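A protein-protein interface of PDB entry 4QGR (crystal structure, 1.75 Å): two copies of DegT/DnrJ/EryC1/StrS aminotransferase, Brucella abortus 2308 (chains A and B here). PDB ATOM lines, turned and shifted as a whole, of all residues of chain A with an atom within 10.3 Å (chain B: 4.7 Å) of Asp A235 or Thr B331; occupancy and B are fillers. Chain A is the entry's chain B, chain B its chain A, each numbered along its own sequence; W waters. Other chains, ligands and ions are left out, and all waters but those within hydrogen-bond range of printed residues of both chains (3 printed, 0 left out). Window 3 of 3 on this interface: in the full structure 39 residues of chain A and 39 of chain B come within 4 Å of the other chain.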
ATOM      1  N   SER A 223     -26.283 -10.194  10.820  1.00  0.00           N
ATOM      2  CA  SER A 223     -25.428  -9.251  11.484  1.00  0.00           C
ATOM      3  C   SER A 223     -25.776  -7.808  11.107  1.00  0.00           C
ATOM      4  O   SER A 223     -25.949  -6.949  11.961  1.00  0.00           O
ATOM      5  CB  SER A 223     -23.980  -9.562  11.070  1.00  0.00           C
ATOM      6  OG  SER A 223     -23.111  -8.501  11.463  1.00  0.00           O
ATOM      7  N   PHE A 226     -28.779  -6.031  12.723  1.00  0.00           N
ATOM      8  CA  PHE A 226     -28.622  -5.687  14.109  1.00  0.00           C
ATOM      9  C   PHE A 226     -27.247  -5.039  14.362  1.00  0.00           C
ATOM     10  O   PHE A 226     -26.406  -5.585  15.063  1.00  0.00           O
ATOM     11  CB  PHE A 226     -28.849  -6.917  14.984  1.00  0.00           C
ATOM     12  CG  PHE A 226     -28.833  -6.623  16.479  1.00  0.00           C
ATOM     13  CD1 PHE A 226     -29.399  -5.459  16.997  1.00  0.00           C
ATOM     14  CD2 PHE A 226     -28.230  -7.501  17.356  1.00  0.00           C
ATOM     15  CE1 PHE A 226     -29.383  -5.200  18.365  1.00  0.00           C
ATOM     16  CE2 PHE A 226     -28.215  -7.250  18.723  1.00  0.00           C
ATOM     17  CZ  PHE A 226     -28.798  -6.101  19.226  1.00  0.00           C
ATOM     18  N   HIS A 227     -27.049  -3.889  13.710  1.00  0.00           N
ATOM     19  CA  HIS A 227     -25.859  -3.029  13.885  1.00  0.00           C
ATOM     20  C   HIS A 227     -24.535  -3.710  13.632  1.00  0.00           C
ATOM     21  O   HIS A 227     -23.507  -3.297  14.160  1.00  0.00           O
ATOM     22  CB  HIS A 227     -25.870  -2.410  15.282  1.00  0.00           C
ATOM     23  CG  HIS A 227     -27.149  -1.720  15.608  1.00  0.00           C
ATOM     24  ND1 HIS A 227     -27.481  -0.487  15.083  1.00  0.00           N
ATOM     25  CD2 HIS A 227     -28.198  -2.098  16.372  1.00  0.00           C
ATOM     26  CE1 HIS A 227     -28.670  -0.129  15.536  1.00  0.00           C
ATOM     27  NE2 HIS A 227     -29.133  -1.097  16.300  1.00  0.00           N
ATOM     28  N   GLY A 228     -24.527  -4.695  12.751  1.00  0.00           N
ATOM     29  CA  GLY A 228     -23.269  -5.337  12.368  1.00  0.00           C
ATOM     30  C   GLY A 228     -22.664  -6.221  13.441  1.00  0.00           C
ATOM     31  O   GLY A 228     -21.438  -6.346  13.523  1.00  0.00           O
ATOM     32  N   LYS A 229     -23.510  -6.861  14.230  1.00  0.00           N
ATOM     33  CA  LYS A 229     -23.053  -7.699  15.360  1.00  0.00           C
ATOM     34  C   LYS A 229     -22.056  -8.739  14.889  1.00  0.00           C
ATOM     35  O   LYS A 229     -22.237  -9.350  13.844  1.00  0.00           O
ATOM     36  CB  LYS A 229     -24.203  -8.505  16.011  1.00  0.00           C
ATOM     37  N   GLY A 230     -21.035  -8.952  15.686  1.00  0.00           N
ATOM     38  CA  GLY A 230     -20.050  -9.984  15.417  1.00  0.00           C
ATOM     39  C   GLY A 230     -20.515 -11.284  16.021  1.00  0.00           C
ATOM     40  O   GLY A 230     -21.683 -11.483  16.305  1.00  0.00           O
ATOM     41  N   GLU A 231     -19.567 -12.179  16.240  1.00  0.00           N
ATOM     42  CA  GLU A 231     -19.885 -13.473  16.854  1.00  0.00           C
ATOM     43  C   GLU A 231     -20.287 -13.351  18.325  1.00  0.00           C
ATOM     44  O   GLU A 231     -20.866 -14.284  18.880  1.00  0.00           O
ATOM     45  CB  GLU A 231     -18.690 -14.434  16.697  1.00  0.00           C
ATOM     46  CG  GLU A 231     -18.281 -14.629  15.241  1.00  0.00           C
ATOM     47  CD  GLU A 231     -19.342 -15.306  14.410  1.00  0.00           C
ATOM     48  OE1 GLU A 231     -20.184 -16.040  15.009  1.00  0.00           O
ATOM     49  OE2 GLU A 231     -19.333 -15.114  13.159  1.00  0.00           O
ATOM     50  N   THR A 232     -19.977 -12.222  18.964  1.00  0.00           N
ATOM     51  CA  THR A 232     -20.416 -11.976  20.332  1.00  0.00           C
ATOM     52  C   THR A 232     -21.472 -10.896  20.400  1.00  0.00           C
ATOM     53  O   THR A 232     -21.863 -10.286  19.396  1.00  0.00           O
ATOM     54  CB  THR A 232     -19.281 -11.482  21.247  1.00  0.00           C
ATOM     55  OG1 THR A 232     -18.987 -10.106  20.924  1.00  0.00           O
ATOM     56  CG2 THR A 232     -18.038 -12.347  21.129  1.00  0.00           C
ATOM     57  N   GLN A 233     -21.899 -10.646  21.631  1.00  0.00           N
ATOM     58  CA  GLN A 233     -22.938  -9.676  21.960  1.00  0.00           C
ATOM     59  C   GLN A 233     -22.388  -8.254  22.124  1.00  0.00           C
ATOM     60  O   GLN A 233     -23.150  -7.264  22.153  1.00  0.00           O
ATOM     61  CB  GLN A 233     -23.557 -10.134  23.294  1.00  0.00           C
ATOM     62  CG  GLN A 233     -24.875  -9.487  23.662  1.00  0.00           C
ATOM     63  CD  GLN A 233     -25.322  -9.835  25.073  1.00  0.00           C
ATOM     64  OE1 GLN A 233     -24.939 -10.876  25.640  1.00  0.00           O
ATOM     65  NE2 GLN A 233     -26.140  -8.963  25.648  1.00  0.00           N
ATOM     66  N   TYR A 234     -21.069  -8.139  22.233  1.00  0.00           N
ATOM     67  CA  TYR A 234     -20.486  -6.897  22.677  1.00  0.00           C
ATOM     68  C   TYR A 234     -19.492  -6.254  21.716  1.00  0.00           C
ATOM     69  O   TYR A 234     -18.870  -5.274  22.091  1.00  0.00           O
ATOM     70  CB  TYR A 234     -19.773  -7.151  23.986  1.00  0.00           C
ATOM     71  CG  TYR A 234     -20.652  -7.681  25.068  1.00  0.00           C
ATOM     72  CD1 TYR A 234     -21.768  -6.954  25.492  1.00  0.00           C
ATOM     73  CD2 TYR A 234     -20.358  -8.892  25.707  1.00  0.00           C
ATOM     74  CE1 TYR A 234     -22.572  -7.420  26.521  1.00  0.00           C
ATOM     75  CE2 TYR A 234     -21.165  -9.380  26.728  1.00  0.00           C
ATOM     76  CZ  TYR A 234     -22.266  -8.632  27.137  1.00  0.00           C
ATOM     77  OH  TYR A 234     -23.074  -9.089  28.156  1.00  0.00           O
ATOM     78  N   ASP A 235     -19.344  -6.796  20.509  1.00  0.00           N
ATOM     79  CA  ASP A 235     -18.389  -6.241  19.550  1.00  0.00           C
ATOM     80  C   ASP A 235     -18.946  -6.296  18.163  1.00  0.00           C
ATOM     81  O   ASP A 235     -18.944  -7.367  17.540  1.00  0.00           O
ATOM     82  CB  ASP A 235     -17.097  -7.055  19.592  1.00  0.00           C
ATOM     83  CG  ASP A 235     -16.026  -6.481  18.684  1.00  0.00           C
ATOM     84  OD1 ASP A 235     -15.771  -5.285  18.796  1.00  0.00           O
ATOM     85  OD2 ASP A 235     -15.441  -7.224  17.866  1.00  0.00           O
ATOM     86  N   ASN A 236     -19.399  -5.158  17.650  1.00  0.00           N
ATOM     87  CA  ASN A 236     -19.814  -5.067  16.291  1.00  0.00           C
ATOM     88  C   ASN A 236     -18.613  -5.075  15.351  1.00  0.00           C
ATOM     89  O   ASN A 236     -17.614  -4.396  15.623  1.00  0.00           O
ATOM     90  CB  ASN A 236     -20.641  -3.807  16.086  1.00  0.00           C
ATOM     91  CG  ASN A 236     -21.921  -3.827  16.891  1.00  0.00           C
ATOM     92  OD1 ASN A 236     -22.488  -4.895  17.166  1.00  0.00           O
ATOM     93  ND2 ASN A 236     -22.427  -2.636  17.236  1.00  0.00           N
ATOM     94  N   VAL A 237     -18.729  -5.799  14.235  1.00  0.00           N
ATOM     95  CA  VAL A 237     -17.610  -5.953  13.341  1.00  0.00           C
ATOM     96  C   VAL A 237     -17.783  -5.269  12.004  1.00  0.00           C
ATOM     97  O   VAL A 237     -16.826  -5.166  11.251  1.00  0.00           O
ATOM     98  CB  VAL A 237     -17.244  -7.425  13.153  1.00  0.00           C
ATOM     99  CG1 VAL A 237     -16.946  -8.019  14.532  1.00  0.00           C
ATOM    100  CG2 VAL A 237     -18.335  -8.148  12.374  1.00  0.00           C
ATOM    101  N   ARG A 238     -18.970  -4.754  11.737  1.00  0.00           N
ATOM    102  CA  ARG A 238     -19.236  -4.073  10.491  1.00  0.00           C
ATOM    103  C   ARG A 238     -20.279  -2.991  10.782  1.00  0.00           C
ATOM    104  O   ARG A 238     -20.916  -3.016  11.829  1.00  0.00           O
ATOM    105  CB  ARG A 238     -19.707  -5.050   9.395  1.00  0.00           C
ATOM    106  CG  ARG A 238     -20.955  -5.864   9.720  1.00  0.00           C
ATOM    107  CD  ARG A 238     -21.336  -6.814   8.577  1.00  0.00           C
ATOM    108  NE  ARG A 238     -20.264  -7.765   8.288  1.00  0.00           N
ATOM    109  CZ  ARG A 238     -20.050  -8.897   8.944  1.00  0.00           C
ATOM    110  NH1 ARG A 238     -20.829  -9.267   9.942  1.00  0.00           N
ATOM    111  NH2 ARG A 238     -19.025  -9.671   8.589  1.00  0.00           N
ATOM    112  N   ILE A 239     -20.427  -2.065   9.839  1.00  0.00           N
ATOM    113  CA  ILE A 239     -21.501  -1.075   9.934  1.00  0.00           C
ATOM    114  C   ILE A 239     -22.808  -1.784   9.583  1.00  0.00           C
ATOM    115  O   ILE A 239     -22.889  -2.557   8.631  1.00  0.00           O
ATOM    116  CB  ILE A 239     -21.261   0.126   8.996  1.00  0.00           C
ATOM    117  CG1 ILE A 239     -19.948   0.828   9.291  1.00  0.00           C
ATOM    118  CG2 ILE A 239     -22.451   1.120   9.015  1.00  0.00           C
ATOM    119  CD1 ILE A 239     -19.739   1.287  10.723  1.00  0.00           C
ATOM    120  N   LYS B 325     -18.171  -2.811  26.293  1.00  0.00           N
ATOM    121  CA  LYS B 325     -17.117  -2.414  25.361  1.00  0.00           C
ATOM    122  C   LYS B 325     -17.516  -1.066  24.784  1.00  0.00           C
ATOM    123  O   LYS B 325     -18.504  -0.988  24.073  1.00  0.00           O
ATOM    124  CB  LYS B 325     -16.961  -3.463  24.239  1.00  0.00           C
ATOM    125  CG  LYS B 325     -15.546  -3.896  24.036  1.00  0.00           C
ATOM    126  CD  LYS B 325     -15.393  -5.001  23.009  1.00  0.00           C
ATOM    127  CE  LYS B 325     -14.180  -4.717  22.132  1.00  0.00           C
ATOM    128  NZ  LYS B 325     -13.389  -5.957  21.930  1.00  0.00           N
ATOM    129  N   LEU B 329     -13.460   0.914  21.031  1.00  0.00           N
ATOM    130  CA  LEU B 329     -12.710  -0.335  21.115  1.00  0.00           C
ATOM    131  C   LEU B 329     -13.344  -1.452  20.316  1.00  0.00           C
ATOM    132  O   LEU B 329     -12.762  -2.539  20.223  1.00  0.00           O
ATOM    133  CB  LEU B 329     -12.517  -0.759  22.564  1.00  0.00           C
ATOM    134  CG  LEU B 329     -11.708   0.210  23.408  1.00  0.00           C
ATOM    135  CD1 LEU B 329     -11.754  -0.326  24.828  1.00  0.00           C
ATOM    136  CD2 LEU B 329     -10.291   0.475  22.931  1.00  0.00           C
ATOM    137  N   GLN B 330     -14.522  -1.225  19.734  1.00  0.00           N
ATOM    138  CA  GLN B 330     -15.169  -2.290  18.971  1.00  0.00           C
ATOM    139  C   GLN B 330     -14.610  -2.299  17.578  1.00  0.00           C
ATOM    140  O   GLN B 330     -14.224  -1.257  17.045  1.00  0.00           O
ATOM    141  CB  GLN B 330     -16.693  -2.140  18.934  1.00  0.00           C
ATOM    142  CG  GLN B 330     -17.319  -2.273  20.328  1.00  0.00           C
ATOM    143  CD  GLN B 330     -18.820  -2.292  20.311  1.00  0.00           C
ATOM    144  OE1 GLN B 330     -19.437  -2.736  19.345  1.00  0.00           O
ATOM    145  NE2 GLN B 330     -19.435  -1.768  21.387  1.00  0.00           N
ATOM    146  N   THR B 331     -14.587  -3.484  16.991  1.00  0.00           N
ATOM    147  CA  THR B 331     -13.983  -3.724  15.685  1.00  0.00           C
ATOM    148  C   THR B 331     -14.442  -2.773  14.617  1.00  0.00           C
ATOM    149  O   THR B 331     -13.627  -2.279  13.817  1.00  0.00           O
ATOM    150  CB  THR B 331     -14.204  -5.214  15.237  1.00  0.00           C
ATOM    151  OG1 THR B 331     -13.624  -6.096  16.210  1.00  0.00           O
ATOM    152  CG2 THR B 331     -13.614  -5.520  13.885  1.00  0.00           C
ATOM    153  N   ALA B 332     -15.735  -2.542  14.536  1.00  0.00           N
ATOM    154  CA  ALA B 332     -16.244  -1.711  13.444  1.00  0.00           C
ATOM    155  C   ALA B 332     -15.786  -0.266  13.519  1.00  0.00           C
ATOM    156  O   ALA B 332     -15.808   0.404  12.505  1.00  0.00           O
ATOM    157  CB  ALA B 332     -17.747  -1.723  13.426  1.00  0.00           C
ATOM    158  N   TYR B 333     -15.438   0.234  14.701  1.00  0.00           N
ATOM    159  CA  TYR B 333     -15.174   1.695  14.866  1.00  0.00           C
ATOM    160  C   TYR B 333     -13.793   2.060  15.375  1.00  0.00           C
ATOM    161  O   TYR B 333     -13.505   3.241  15.553  1.00  0.00           O
ATOM    162  CB  TYR B 333     -16.245   2.350  15.827  1.00  0.00           C
ATOM    163  CG  TYR B 333     -17.617   1.711  15.714  1.00  0.00           C
ATOM    164  CD1 TYR B 333     -18.500   1.987  14.668  1.00  0.00           C
ATOM    165  CD2 TYR B 333     -18.041   0.827  16.670  1.00  0.00           C
ATOM    166  CE1 TYR B 333     -19.757   1.330  14.584  1.00  0.00           C
ATOM    167  CE2 TYR B 333     -19.264   0.176  16.587  1.00  0.00           C
ATOM    168  CZ  TYR B 333     -20.118   0.408  15.557  1.00  0.00           C
ATOM    169  OH  TYR B 333     -21.307  -0.340  15.570  1.00  0.00           O
ATOM    170  N   LYS B 334     -12.956   1.069  15.626  1.00  0.00           N
ATOM    171  CA  LYS B 334     -11.723   1.293  16.345  1.00  0.00           C
ATOM    172  C   LYS B 334     -10.662   1.993  15.505  1.00  0.00           C
ATOM    173  O   LYS B 334      -9.649   2.434  16.054  1.00  0.00           O
ATOM    174  CB  LYS B 334     -11.172  -0.027  16.911  1.00  0.00           C
ATOM    175  CG  LYS B 334     -10.652  -1.001  15.895  1.00  0.00           C
ATOM    176  CD  LYS B 334     -10.259  -2.293  16.597  1.00  0.00           C
ATOM    177  CE  LYS B 334      -9.657  -3.308  15.646  1.00  0.00           C
ATOM    178  NZ  LYS B 334      -9.117  -4.427  16.475  1.00  0.00           N
HETATM  179  O   HOH W   1     -21.943  -3.645  20.356  1.00  0.00           O
HETATM  180  O   HOH W   2     -22.037  -0.855  13.248  1.00  0.00           O
HETATM  181  O   HOH W   3     -20.326  -3.647  24.344  1.00  0.00           O
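The side-chain hydroxyl of Tyr B333 is in hydrogen-bond range of the side-chain amide nitrogen of Asn A236. The backbone NH (N) of Asn A236 sits at hydrogen-bond distance from the side-chain amide oxygen (OE1) of Gln B330. The backbone NH of Ala B332 lies within hydrogen-bond range of the backbone carbonyl oxygen of Asn A236. OG1 of Thr B331 lies within hydrogen-bond range of OD2 of Asp A235, 2.7 Å away. N of Thr B331 is in hydrogen-bond range of O of Asn A236 (3.4 Å). The side-chain amino group (NZ) of Lys B325 lies within salt-bridge range of the side-chain carboxylate (OD1) of Asp A235, 3.99 Å away.
The backbone carbonyl oxygen of Asp A235 lies within hydrogen-bond range of the backbone NH of Gly A230 (3.2 Å). The backbone carbonyl oxygen (O) of Gly A228 sits at hydrogen-bond distance from the backbone NH (N) of Val A237 (2.9 Å). O of Lys B325 is in hydrogen-bond range of NE2 of Gln B330, at 2.9 Å. The side-chain hydroxyl of Thr A232 lies within hydrogen-bond range of the backbone NH of Tyr A234. The guanidinium group (NH1) of Arg A238 lies within hydrogen-bond range of the side-chain hydroxyl (OG) of Ser A223. OG1 of Thr A232 sits at hydrogen-bond distance from N of Asp A235 (3.4 Å).
Among the printed residues, pairs that only touch across the chains: Asp A235 with Gln B330 (3.1 Å), Tyr A234 with Lys B325 (3.4 Å), Tyr A234 with Gln B330 (3.5 Å), Arg A238 with Ala B332 (3.7 Å), Val A237 with Ala B332 (3.8 Å), Ile A239 with Tyr B333 (3.9 Å), His A227 with Tyr B333 (3.9 Å) and Val A237 with Thr B331 (3.97 Å).
Of the printed residues of chain B, His A227 touches Tyr B333 (3.9 Å). Gly A228 touches none of the printed residues of chain B. Gln A233 touches none of the printed residues of chain B. Printed residues of chain B within 4 Å of Tyr A234: Lys B325 (3.4 Å) and Gln B330 (3.5 Å). Of the printed residues of chain B, Asn A236 touches Gln B330, Thr B331, Ala B332 and Tyr B333. Of the printed residues of chain B, Arg A238 touches Ala B332 (3.7 Å). Of the printed residues of chain A, Lys B325 touches Tyr A234 and Asp A235. Gln B330 touches just these residues of chain A: Tyr A234 (3.5 Å), Asp A235 (3.1 Å) and Asn A236 (3.0 Å). Thr B331 touches three residues of chain A. Ala B332 touches just these residues of chain A: Asn A236 (2.9 Å), Val A237 (3.8 Å) and Arg A238 (3.7 Å). The nearest residue of chain B that does not touch Asp A235 is Leu B329 (4.3 Å). The nearest printed residue of chain B that does not touch Val A237 is Gln B330 (6.0 Å).
Hydrophobic or aromatic side chains of chain B that line the printed part of chain A: Ala B332 and Tyr B333. Of the 15 printed residues of chain A, 7 touch a printed residue of chain B. Hydrophobic or aromatic side chains of chain A within 4 Å of the printed part of chain B: Val A237 and Ile A239.
No position is printed for both chains.
Water W2 lies within hydrogen-bond range of OH of Tyr B333 (2.5 Å), O of Arg A238 (2.8 Å) and O of His A227 (3.0 Å). Water W1 lies within hydrogen-bond range of the side-chain amide oxygen of Gln B330 (2.9 Å) and the side-chain amide nitrogen of Asn A236 (3.3 Å). Water W3 lies within hydrogen-bond range of the backbone NH (N) of Lys B325 (3.0 Å) and the backbone carbonyl oxygen (O) of Tyr A234 (3.1 Å).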
